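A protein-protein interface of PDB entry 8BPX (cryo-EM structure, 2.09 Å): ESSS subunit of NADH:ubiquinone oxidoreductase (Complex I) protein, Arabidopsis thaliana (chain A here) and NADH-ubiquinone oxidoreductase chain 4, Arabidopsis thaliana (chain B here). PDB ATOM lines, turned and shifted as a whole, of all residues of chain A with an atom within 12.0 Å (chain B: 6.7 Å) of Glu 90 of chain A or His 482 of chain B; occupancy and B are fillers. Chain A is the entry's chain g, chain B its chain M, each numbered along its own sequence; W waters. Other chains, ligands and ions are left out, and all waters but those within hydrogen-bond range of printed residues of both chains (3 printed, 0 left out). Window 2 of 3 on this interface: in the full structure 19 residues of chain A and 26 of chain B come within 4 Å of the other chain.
The side-chain sulfur (SG) of Cys 480 of chain B is in hydrogen-bond range of the side-chain amino group (NZ) of Lys 84 of chain A (3.6 Å).
The side-chain hydroxyl of Ser 61 of chain B sits at hydrogen-bond distance from the backbone NH of Ser 88 of chain A, 3.3 Å away.
ND1 of His 482 of chain B lies within hydrogen-bond range of OE1 of Glu 90 of chain A, 2.5 Å away.
The side-chain hydroxyl (OG) of Ser 486 of chain B lies within hydrogen-bond range of the backbone carbonyl oxygen (O) of His 482 of chain B (3.1 Å).
The backbone carbonyl oxygen of Leu 478 of chain B sits at hydrogen-bond distance from a ring nitrogen (ND1) of His 482 of chain B (3.3 Å).
The backbone carbonyl oxygen (O) of Thr 483 of chain B lies within hydrogen-bond range of the side-chain amide nitrogen (ND2) of Asn 487 of chain B (3.2 Å).
The side-chain hydroxyl of Ser 88 of chain A is in hydrogen-bond range of the side-chain hydroxyl of Thr 91 of chain A (2.8 Å).
The side-chain carboxylate of Asp 86 of chain A lies within hydrogen-bond range of the side-chain hydroxyl of Ser 88 of chain A (3.2 Å).
OG1 of Thr 483 of chain B lies within hydrogen-bond range of O of Ser 61 of chain B (3.0 Å).
Among the printed residues, pairs that only touch across the chains: Leu 87 of chain A with Ser 61 of chain B (3.4 Å), Ile 89 of chain A with Thr 483 of chain B (3.6 Å) and Ile 89 of chain A with Ser 61 of chain B (3.9 Å).
Of the printed residues of chain B, Lys 84 of chain A touches Cys 480 (3.6 Å).
Printed residues of chain B within 4 Å of Leu 87 of chain A: Ser 61.
Of the printed residues of chain B, Ile 89 of chain A touches Ser 61 (3.9 Å) and Thr 483 (3.6 Å).
Printed residues of chain B within 4 Å of Glu 90 of chain A: His 482.
No residue of chain A comes within 4 Å of Ile 328 of chain B.
No residue of chain A comes within 4 Å of Gly 332 of chain B.
No residue of chain A comes within 4 Å of Leu 478 of chain B.
No residue of chain A comes within 4 Å of Asp 479 of chain B.
Cys 480 of chain B touches just one residue of chain A: Lys 84 (3.6 Å).
No residue of chain A comes within 4 Å of Met 481 of chain B.
Printed residues of chain A within 4 Å of His 482 of chain B: Glu 90.
No residue of chain A comes within 4 Å of Ser 484 of chain B.
No residue of chain A comes within 4 Å of Val 485 of chain B.
No residue of chain A comes within 4 Å of Ser 486 of chain B.
Of the 18 printed residues of chain B, 4 touch a printed residue of chain A.
Water W2 bridges the side-chain hydroxyl of Ser 88 of chain A (2.6 Å) and the side-chain carboxylate of Asp 479 of chain B (3.1 Å).
Water W1 lies within hydrogen-bond range of the backbone carbonyl oxygen (O) of Ser 61 of chain B, the backbone carbonyl oxygen (O) of Asp 479 of chain B, the backbone NH (N) of Ile 89 of chain A and the side-chain hydroxyl (OG1) of Thr 483 of chain B.
Water W3 lies within hydrogen-bond range of OE1 of Glu 90 of chain A (2.8 Å) and ND1 of His 482 of chain B (3.4 Å).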
ATOM      1  N   LYS A  84       6.714 -25.782  13.683  1.00  0.00           N
ATOM      2  CA  LYS A  84       6.256 -24.379  13.800  1.00  0.00           C
ATOM      3  C   LYS A  84       7.092 -23.545  12.827  1.00  0.00           C
ATOM      4  O   LYS A  84       8.296 -23.826  12.671  1.00  0.00           O
ATOM      5  CB  LYS A  84       6.313 -23.871  15.245  1.00  0.00           C
ATOM      6  CG  LYS A  84       7.687 -23.547  15.813  1.00  0.00           C
ATOM      7  CD  LYS A  84       7.659 -23.286  17.302  1.00  0.00           C
ATOM      8  CE  LYS A  84       6.901 -22.030  17.685  1.00  0.00           C
ATOM      9  NZ  LYS A  84       7.592 -21.278  18.762  1.00  0.00           N
ATOM     10  N   PRO A  85       6.499 -22.509  12.214  1.00  0.00           N
ATOM     11  CA  PRO A  85       7.270 -21.596  11.375  1.00  0.00           C
ATOM     12  C   PRO A  85       8.412 -20.986  12.205  1.00  0.00           C
ATOM     13  O   PRO A  85       8.242 -20.769  13.394  1.00  0.00           O
ATOM     14  CB  PRO A  85       6.194 -20.585  10.979  1.00  0.00           C
ATOM     15  CG  PRO A  85       5.177 -20.645  12.081  1.00  0.00           C
ATOM     16  CD  PRO A  85       5.101 -22.121  12.382  1.00  0.00           C
ATOM     17  N   ASP A  86       9.537 -20.698  11.567  1.00  0.00           N
ATOM     18  CA  ASP A  86      10.610 -19.920  12.182  1.00  0.00           C
ATOM     19  C   ASP A  86      10.264 -18.444  12.037  1.00  0.00           C
ATOM     20  O   ASP A  86      10.368 -17.870  10.952  1.00  0.00           O
ATOM     21  CB  ASP A  86      11.950 -20.256  11.541  1.00  0.00           C
ATOM     22  CG  ASP A  86      13.099 -19.476  12.142  1.00  0.00           C
ATOM     23  OD1 ASP A  86      14.137 -19.340  11.468  1.00  0.00           O
ATOM     24  OD2 ASP A  86      12.974 -19.005  13.291  1.00  0.00           O
ATOM     25  N   LEU A  87       9.914 -17.823  13.156  1.00  0.00           N
ATOM     26  CA  LEU A  87       9.455 -16.419  13.163  1.00  0.00           C
ATOM     27  C   LEU A  87      10.441 -15.556  13.948  1.00  0.00           C
ATOM     28  O   LEU A  87      10.184 -14.386  14.104  1.00  0.00           O
ATOM     29  CB  LEU A  87       8.041 -16.359  13.744  1.00  0.00           C
ATOM     30  CG  LEU A  87       6.978 -17.128  12.966  1.00  0.00           C
ATOM     31  CD1 LEU A  87       5.624 -16.992  13.639  1.00  0.00           C
ATOM     32  CD2 LEU A  87       6.912 -16.654  11.523  1.00  0.00           C
ATOM     33  N   SER A  88      11.580 -16.105  14.339  1.00  0.00           N
ATOM     34  CA  SER A  88      12.510 -15.390  15.196  1.00  0.00           C
ATOM     35  C   SER A  88      12.962 -14.089  14.538  1.00  0.00           C
ATOM     36  O   SER A  88      13.068 -13.988  13.313  1.00  0.00           O
ATOM     37  CB  SER A  88      13.712 -16.275  15.519  1.00  0.00           C
ATOM     38  OG  SER A  88      14.536 -16.453  14.384  1.00  0.00           O
ATOM     39  N   ILE A  89      13.211 -13.078  15.374  1.00  0.00           N
ATOM     40  CA  ILE A  89      13.672 -11.788  14.869  1.00  0.00           C
ATOM     41  C   ILE A  89      15.022 -11.939  14.181  1.00  0.00           C
ATOM     42  O   ILE A  89      15.298 -11.262  13.186  1.00  0.00           O
ATOM     43  CB  ILE A  89      13.719 -10.750  16.011  1.00  0.00           C
ATOM     44  CG1 ILE A  89      14.319  -9.435  15.522  1.00  0.00           C
ATOM     45  CG2 ILE A  89      14.531 -11.260  17.184  1.00  0.00           C
ATOM     46  CD1 ILE A  89      13.367  -8.604  14.722  1.00  0.00           C
ATOM     47  N   GLU A  90      15.871 -12.838  14.683  1.00  0.00           N
ATOM     48  CA  GLU A  90      17.173 -13.070  14.068  1.00  0.00           C
ATOM     49  C   GLU A  90      17.023 -13.543  12.625  1.00  0.00           C
ATOM     50  O   GLU A  90      17.704 -13.043  11.724  1.00  0.00           O
ATOM     51  CB  GLU A  90      17.960 -14.092  14.887  1.00  0.00           C
ATOM     52  CG  GLU A  90      18.320 -13.635  16.283  1.00  0.00           C
ATOM     53  CD  GLU A  90      17.357 -14.146  17.346  1.00  0.00           C
ATOM     54  OE1 GLU A  90      17.758 -14.205  18.521  1.00  0.00           O
ATOM     55  OE2 GLU A  90      16.195 -14.469  17.015  1.00  0.00           O
ATOM     56  N   THR A  91      16.124 -14.498  12.386  1.00  0.00           N
ATOM     57  CA  THR A  91      15.935 -15.025  11.037  1.00  0.00           C
ATOM     58  C   THR A  91      15.380 -13.968  10.091  1.00  0.00           C
ATOM     59  O   THR A  91      15.826 -13.862   8.945  1.00  0.00           O
ATOM     60  CB  THR A  91      15.015 -16.244  11.072  1.00  0.00           C
ATOM     61  OG1 THR A  91      15.609 -17.266  11.881  1.00  0.00           O
ATOM     62  CG2 THR A  91      14.781 -16.783   9.672  1.00  0.00           C
ATOM     63  N   TRP A  92      14.397 -13.187  10.548  1.00  0.00           N
ATOM     64  CA  TRP A  92      13.855 -12.124   9.709  1.00  0.00           C
ATOM     65  C   TRP A  92      14.900 -11.051   9.428  1.00  0.00           C
ATOM     66  O   TRP A  92      15.004 -10.556   8.301  1.00  0.00           O
ATOM     67  CB  TRP A  92      12.616 -11.509  10.360  1.00  0.00           C
ATOM     68  CG  TRP A  92      12.133 -10.269   9.670  1.00  0.00           C
ATOM     69  CD1 TRP A  92      11.194 -10.195   8.691  1.00  0.00           C
ATOM     70  CD2 TRP A  92      12.558  -8.923   9.917  1.00  0.00           C
ATOM     71  NE1 TRP A  92      11.014  -8.894   8.302  1.00  0.00           N
ATOM     72  CE2 TRP A  92      11.843  -8.091   9.040  1.00  0.00           C
ATOM     73  CE3 TRP A  92      13.482  -8.344  10.791  1.00  0.00           C
ATOM     74  CZ2 TRP A  92      12.015  -6.710   9.012  1.00  0.00           C
ATOM     75  CZ3 TRP A  92      13.657  -6.976  10.757  1.00  0.00           C
ATOM     76  CH2 TRP A  92      12.923  -6.173   9.878  1.00  0.00           C
ATOM     77  N   ALA A  93      15.678 -10.673  10.442  1.00  0.00           N
ATOM     78  CA  ALA A  93      16.678  -9.630  10.247  1.00  0.00           C
ATOM     79  C   ALA A  93      17.837 -10.114   9.382  1.00  0.00           C
ATOM     80  O   ALA A  93      18.419  -9.319   8.641  1.00  0.00           O
ATOM     81  CB  ALA A  93      17.186  -9.122  11.593  1.00  0.00           C
ATOM     82  N   HIS A  94      18.218 -11.374   9.495  1.00  0.00           N
ATOM     83  CA  HIS A  94      19.282 -11.960   8.626  1.00  0.00           C
ATOM     84  C   HIS A  94      18.930 -11.823   7.121  1.00  0.00           C
ATOM     85  O   HIS A  94      19.736 -11.328   6.395  1.00  0.00           O
ATOM     86  CB  HIS A  94      19.665 -13.378   9.072  1.00  0.00           C
ATOM     87  CG  HIS A  94      20.791 -13.944   8.277  1.00  0.00           C
ATOM     88  ND1 HIS A  94      22.094 -13.861   8.689  1.00  0.00           N
ATOM     89  CD2 HIS A  94      20.819 -14.554   7.080  1.00  0.00           C
ATOM     90  CE1 HIS A  94      22.868 -14.422   7.800  1.00  0.00           C
ATOM     91  NE2 HIS A  94      22.118 -14.848   6.806  1.00  0.00           N
ATOM     92  N   GLN A  95      17.705 -12.190   6.745  1.00  0.00           N
ATOM     93  CA  GLN A  95      17.298 -12.035   5.352  1.00  0.00           C
ATOM     94  C   GLN A  95      17.248 -10.569   4.953  1.00  0.00           C
ATOM     95  O   GLN A  95      17.597 -10.210   3.824  1.00  0.00           O
ATOM     96  CB  GLN A  95      15.939 -12.701   5.115  1.00  0.00           C
ATOM     97  CG  GLN A  95      15.428 -12.756   3.665  1.00  0.00           C
ATOM     98  CD  GLN A  95      14.152 -13.572   3.451  1.00  0.00           C
ATOM     99  OE1 GLN A  95      13.640 -14.215   4.369  1.00  0.00           O
ATOM    100  NE2 GLN A  95      13.628 -13.528   2.229  1.00  0.00           N
ATOM    101  N   LYS A  96      16.807  -9.707   5.869  1.00  0.00           N
ATOM    102  CA  LYS A  96      16.795  -8.273   5.613  1.00  0.00           C
ATOM    103  C   LYS A  96      18.212  -7.718   5.485  1.00  0.00           C
ATOM    104  O   LYS A  96      18.470  -6.854   4.640  1.00  0.00           O
ATOM    105  CB  LYS A  96      16.032  -7.571   6.737  1.00  0.00           C
ATOM    106  CG  LYS A  96      14.512  -7.564   6.607  1.00  0.00           C
ATOM    107  CD  LYS A  96      14.032  -6.547   5.593  1.00  0.00           C
ATOM    108  CE  LYS A  96      12.669  -6.913   5.024  1.00  0.00           C
ATOM    109  NZ  LYS A  96      12.538  -8.357   4.750  1.00  0.00           N
ATOM    110  N   ALA A  97      19.141  -8.203   6.313  1.00  0.00           N
ATOM    111  CA  ALA A  97      20.524  -7.738   6.247  1.00  0.00           C
ATOM    112  C   ALA A  97      21.186  -8.135   4.931  1.00  0.00           C
ATOM    113  O   ALA A  97      21.925  -7.338   4.335  1.00  0.00           O
ATOM    114  CB  ALA A  97      21.316  -8.291   7.429  1.00  0.00           C
ATOM    115  N   LEU A  98      21.031  -9.399   4.519  1.00  0.00           N
ATOM    116  CA  LEU A  98      21.562  -9.859   3.204  1.00  0.00           C
ATOM    117  C   LEU A  98      21.135  -8.899   2.082  1.00  0.00           C
ATOM    118  O   LEU A  98      22.013  -8.321   1.514  1.00  0.00           O
ATOM    119  CB  LEU A  98      21.123 -11.276   2.870  1.00  0.00           C
ATOM    120  CG  LEU A  98      21.811 -12.377   3.667  1.00  0.00           C
ATOM    121  CD1 LEU A  98      21.049 -13.673   3.562  1.00  0.00           C
ATOM    122  CD2 LEU A  98      23.261 -12.552   3.240  1.00  0.00           C
ATOM    123  N   GLU A  99      19.839  -8.647   1.938  1.00  0.00           N
ATOM    124  CA  GLU A  99      19.362  -7.879   0.796  1.00  0.00           C
ATOM    125  C   GLU A  99      19.807  -6.423   0.859  1.00  0.00           C
ATOM    126  O   GLU A  99      19.934  -5.774  -0.182  1.00  0.00           O
ATOM    127  CB  GLU A  99      17.839  -7.988   0.694  1.00  0.00           C
ATOM    128  CG  GLU A  99      17.057  -6.993   1.509  1.00  0.00           C
ATOM    129  CD  GLU A  99      15.712  -7.538   1.942  1.00  0.00           C
ATOM    130  OE1 GLU A  99      15.469  -8.745   1.737  1.00  0.00           O
ATOM    131  OE2 GLU A  99      14.898  -6.761   2.487  1.00  0.00           O
ATOM    132  N   SER B  61       7.215 -15.841  17.814  1.00  0.00           N
ATOM    133  CA  SER B  61       8.463 -15.340  18.371  1.00  0.00           C
ATOM    134  C   SER B  61       9.032 -14.141  17.615  1.00  0.00           C
ATOM    135  O   SER B  61      10.233 -13.874  17.717  1.00  0.00           O
ATOM    136  CB  SER B  61       9.502 -16.462  18.409  1.00  0.00           C
ATOM    137  OG  SER B  61       9.959 -16.776  17.107  1.00  0.00           O
ATOM    138  N   THR B  63       7.035 -10.945  17.345  1.00  0.00           N
ATOM    139  CA  THR B  63       6.375  -9.717  17.749  1.00  0.00           C
ATOM    140  C   THR B  63       6.864  -9.263  19.118  1.00  0.00           C
ATOM    141  O   THR B  63       7.248 -10.072  19.965  1.00  0.00           O
ATOM    142  CB  THR B  63       4.859  -9.907  17.784  1.00  0.00           C
ATOM    143  OG1 THR B  63       4.253  -8.792  18.441  1.00  0.00           O
ATOM    144  CG2 THR B  63       4.505 -11.171  18.545  1.00  0.00           C
ATOM    145  N   GLY B  88       7.349 -13.343  25.508  1.00  0.00           N
ATOM    146  CA  GLY B  88       8.513 -14.192  25.632  1.00  0.00           C
ATOM    147  C   GLY B  88       9.225 -14.132  26.962  1.00  0.00           C
ATOM    148  O   GLY B  88      10.264 -14.779  27.127  1.00  0.00           O
ATOM    149  N   ILE B 328      20.769  -7.409  26.209  1.00  0.00           N
ATOM    150  CA  ILE B 328      20.232  -8.734  25.750  1.00  0.00           C
ATOM    151  C   ILE B 328      20.804  -9.885  26.557  1.00  0.00           C
ATOM    152  O   ILE B 328      20.016 -10.631  27.052  1.00  0.00           O
ATOM    153  CB  ILE B 328      20.316  -9.008  24.215  1.00  0.00           C
ATOM    154  CG1 ILE B 328      20.011  -7.760  23.377  1.00  0.00           C
ATOM    155  CG2 ILE B 328      19.449 -10.191  23.822  1.00  0.00           C
ATOM    156  CD1 ILE B 328      18.586  -7.292  23.415  1.00  0.00           C
ATOM    157  N   GLN B 329      22.101  -9.892  26.719  1.00  0.00           N
ATOM    158  CA  GLN B 329      22.757 -10.902  27.551  1.00  0.00           C
ATOM    159  C   GLN B 329      22.193 -10.833  28.984  1.00  0.00           C
ATOM    160  O   GLN B 329      21.818 -11.871  29.461  1.00  0.00           O
ATOM    161  CB  GLN B 329      24.276 -10.845  27.443  1.00  0.00           C
ATOM    162  CG  GLN B 329      24.765 -11.056  26.013  1.00  0.00           C
ATOM    163  CD  GLN B 329      24.814  -9.814  25.151  1.00  0.00           C
ATOM    164  OE1 GLN B 329      24.913  -8.696  25.630  1.00  0.00           O
ATOM    165  NE2 GLN B 329      24.772 -10.008  23.849  1.00  0.00           N
ATOM    166  N   GLY B 332      18.207 -11.793  29.013  1.00  0.00           N
ATOM    167  CA  GLY B 332      18.098 -13.176  28.587  1.00  0.00           C
ATOM    168  C   GLY B 332      18.670 -14.141  29.607  1.00  0.00           C
ATOM    169  O   GLY B 332      18.046 -15.154  29.938  1.00  0.00           O
ATOM    170  N   LEU B 402      25.667 -15.736  30.669  1.00  0.00           N
ATOM    171  CA  LEU B 402      25.042 -14.642  29.936  1.00  0.00           C
ATOM    172  C   LEU B 402      24.840 -13.428  30.839  1.00  0.00           C
ATOM    173  O   LEU B 402      24.984 -12.282  30.398  1.00  0.00           O
ATOM    174  CB  LEU B 402      23.724 -15.122  29.334  1.00  0.00           C
ATOM    175  CG  LEU B 402      23.805 -15.728  27.923  1.00  0.00           C
ATOM    176  CD1 LEU B 402      22.429 -15.964  27.335  1.00  0.00           C
ATOM    177  CD2 LEU B 402      24.655 -14.872  26.982  1.00  0.00           C
ATOM    178  N   PHE B 477      14.708 -21.897  23.702  1.00  0.00           N
ATOM    179  CA  PHE B 477      14.143 -20.908  24.612  1.00  0.00           C
ATOM    180  C   PHE B 477      14.468 -19.483  24.173  1.00  0.00           C
ATOM    181  O   PHE B 477      13.583 -18.624  24.136  1.00  0.00           O
ATOM    182  CB  PHE B 477      14.636 -21.176  26.035  1.00  0.00           C
ATOM    183  CG  PHE B 477      14.281 -22.543  26.539  1.00  0.00           C
ATOM    184  CD1 PHE B 477      13.039 -22.784  27.102  1.00  0.00           C
ATOM    185  CD2 PHE B 477      15.174 -23.595  26.421  1.00  0.00           C
ATOM    186  CE1 PHE B 477      12.702 -24.046  27.555  1.00  0.00           C
ATOM    187  CE2 PHE B 477      14.842 -24.855  26.871  1.00  0.00           C
ATOM    188  CZ  PHE B 477      13.602 -25.083  27.438  1.00  0.00           C
ATOM    189  N   LEU B 478      15.726 -19.222  23.815  1.00  0.00           N
ATOM    190  CA  LEU B 478      16.144 -17.857  23.505  1.00  0.00           C
ATOM    191  C   LEU B 478      15.490 -17.329  22.231  1.00  0.00           C
ATOM    192  O   LEU B 478      15.266 -16.121  22.110  1.00  0.00           O
ATOM    193  CB  LEU B 478      17.669 -17.792  23.401  1.00  0.00           C
ATOM    194  CG  LEU B 478      18.418 -17.877  24.734  1.00  0.00           C
ATOM    195  CD1 LEU B 478      19.920 -17.886  24.535  1.00  0.00           C
ATOM    196  CD2 LEU B 478      18.002 -16.750  25.678  1.00  0.00           C
ATOM    197  N   ASP B 479      15.174 -18.209  21.277  1.00  0.00           N
ATOM    198  CA  ASP B 479      14.525 -17.771  20.046  1.00  0.00           C
ATOM    199  C   ASP B 479      13.115 -17.250  20.304  1.00  0.00           C
ATOM    200  O   ASP B 479      12.685 -16.289  19.659  1.00  0.00           O
ATOM    201  CB  ASP B 479      14.485 -18.916  19.036  1.00  0.00           C
ATOM    202  CG  ASP B 479      15.758 -19.023  18.219  1.00  0.00           C
ATOM    203  OD1 ASP B 479      15.773 -19.812  17.255  1.00  0.00           O
ATOM    204  OD2 ASP B 479      16.738 -18.322  18.537  1.00  0.00           O
ATOM    205  N   CYS B 480      12.389 -17.860  21.237  1.00  0.00           N
ATOM    206  CA  CYS B 480      11.046 -17.396  21.555  1.00  0.00           C
ATOM    207  C   CYS B 480      11.037 -16.150  22.432  1.00  0.00           C
ATOM    208  O   CYS B 480       9.981 -15.532  22.579  1.00  0.00           O
ATOM    209  CB  CYS B 480      10.252 -18.511  22.243  1.00  0.00           C
ATOM    210  SG  CYS B 480       9.862 -19.925  21.188  1.00  0.00           S
ATOM    211  N   MET B 481      12.176 -15.756  23.000  1.00  0.00           N
ATOM    212  CA  MET B 481      12.213 -14.657  23.954  1.00  0.00           C
ATOM    213  C   MET B 481      12.789 -13.360  23.404  1.00  0.00           C
ATOM    214  O   MET B 481      12.511 -12.301  23.972  1.00  0.00           O
ATOM    215  CB  MET B 481      13.022 -15.058  25.198  1.00  0.00           C
ATOM    216  CG  MET B 481      12.396 -16.168  26.029  1.00  0.00           C
ATOM    217  SD  MET B 481      13.594 -17.161  26.949  1.00  0.00           S
ATOM    218  CE  MET B 481      14.735 -15.914  27.527  1.00  0.00           C
ATOM    219  N   HIS B 482      13.696 -13.436  22.407  1.00  0.00           N
ATOM    220  CA  HIS B 482      14.468 -12.268  21.912  1.00  0.00           C
ATOM    221  C   HIS B 482      13.625 -11.033  21.562  1.00  0.00           C
ATOM    222  O   HIS B 482      14.053 -10.006  21.933  1.00  0.00           O
ATOM    223  CB  HIS B 482      15.560 -12.621  20.848  1.00  0.00           C
ATOM    224  CG  HIS B 482      16.782 -13.099  21.551  1.00  0.00           C
ATOM    225  ND1 HIS B 482      17.602 -14.064  21.058  1.00  0.00           N
ATOM    226  CD2 HIS B 482      17.248 -12.821  22.785  1.00  0.00           C
ATOM    227  CE1 HIS B 482      18.578 -14.298  21.900  1.00  0.00           C
ATOM    228  NE2 HIS B 482      18.374 -13.564  22.972  1.00  0.00           N
ATOM    229  N   THR B 483      12.519 -11.172  20.885  1.00  0.00           N
ATOM    230  CA  THR B 483      11.752  -9.978  20.525  1.00  0.00           C
ATOM    231  C   THR B 483      11.226  -9.262  21.771  1.00  0.00           C
ATOM    232  O   THR B 483      11.350  -8.036  21.900  1.00  0.00           O
ATOM    233  CB  THR B 483      10.606 -10.344  19.576  1.00  0.00           C
ATOM    234  OG1 THR B 483      11.106 -11.134  18.493  1.00  0.00           O
ATOM    235  CG2 THR B 483       9.951  -9.087  19.013  1.00  0.00           C
ATOM    236  N   SER B 484      10.654 -10.019  22.710  1.00  0.00           N
ATOM    237  CA  SER B 484      10.160  -9.428  23.952  1.00  0.00           C
ATOM    238  C   SER B 484      11.293  -8.808  24.759  1.00  0.00           C
ATOM    239  O   SER B 484      11.168  -7.683  25.259  1.00  0.00           O
ATOM    240  CB  SER B 484       9.432 -10.485  24.784  1.00  0.00           C
ATOM    241  OG  SER B 484       8.254 -10.923  24.141  1.00  0.00           O
ATOM    242  N   VAL B 485      12.411  -9.523  24.883  1.00  0.00           N
ATOM    243  CA  VAL B 485      13.548  -9.011  25.639  1.00  0.00           C
ATOM    244  C   VAL B 485      14.077  -7.737  24.998  1.00  0.00           C
ATOM    245  O   VAL B 485      14.391  -6.758  25.686  1.00  0.00           O
ATOM    246  CB  VAL B 485      14.642 -10.089  25.751  1.00  0.00           C
ATOM    247  CG1 VAL B 485      15.980  -9.464  26.131  1.00  0.00           C
ATOM    248  CG2 VAL B 485      14.238 -11.167  26.741  1.00  0.00           C
ATOM    249  N   SER B 486      14.168  -7.728  23.666  1.00  0.00           N
ATOM    250  CA  SER B 486      14.668  -6.563  22.947  1.00  0.00           C
ATOM    251  C   SER B 486      13.769  -5.359  23.163  1.00  0.00           C
ATOM    252  O   SER B 486      14.254  -4.247  23.384  1.00  0.00           O
ATOM    253  CB  SER B 486      14.779  -6.879  21.457  1.00  0.00           C
ATOM    254  OG  SER B 486      15.907  -7.681  21.189  1.00  0.00           O
ATOM    255  N   ASN B 487      12.455  -5.557  23.100  1.00  0.00           N
ATOM    256  CA  ASN B 487      11.563  -4.421  23.295  1.00  0.00           C
ATOM    257  C   ASN B 487      11.589  -3.936  24.741  1.00  0.00           C
ATOM    258  O   ASN B 487      11.466  -2.733  24.985  1.00  0.00           O
ATOM    259  CB  ASN B 487      10.152  -4.784  22.837  1.00  0.00           C
ATOM    260  CG  ASN B 487       9.916  -4.429  21.375  1.00  0.00           C
ATOM    261  OD1 ASN B 487       9.424  -3.354  21.052  1.00  0.00           O
ATOM    262  ND2 ASN B 487      10.303  -5.332  20.483  1.00  0.00           N
HETATM  263  O   HOH W   1      12.911 -13.784  18.273  1.00  0.00           O
HETATM  264  O   HOH W   2      16.728 -17.620  15.206  1.00  0.00           O
HETATM  265  O   HOH W   3      20.409 -13.924  19.202  1.00  0.00           O
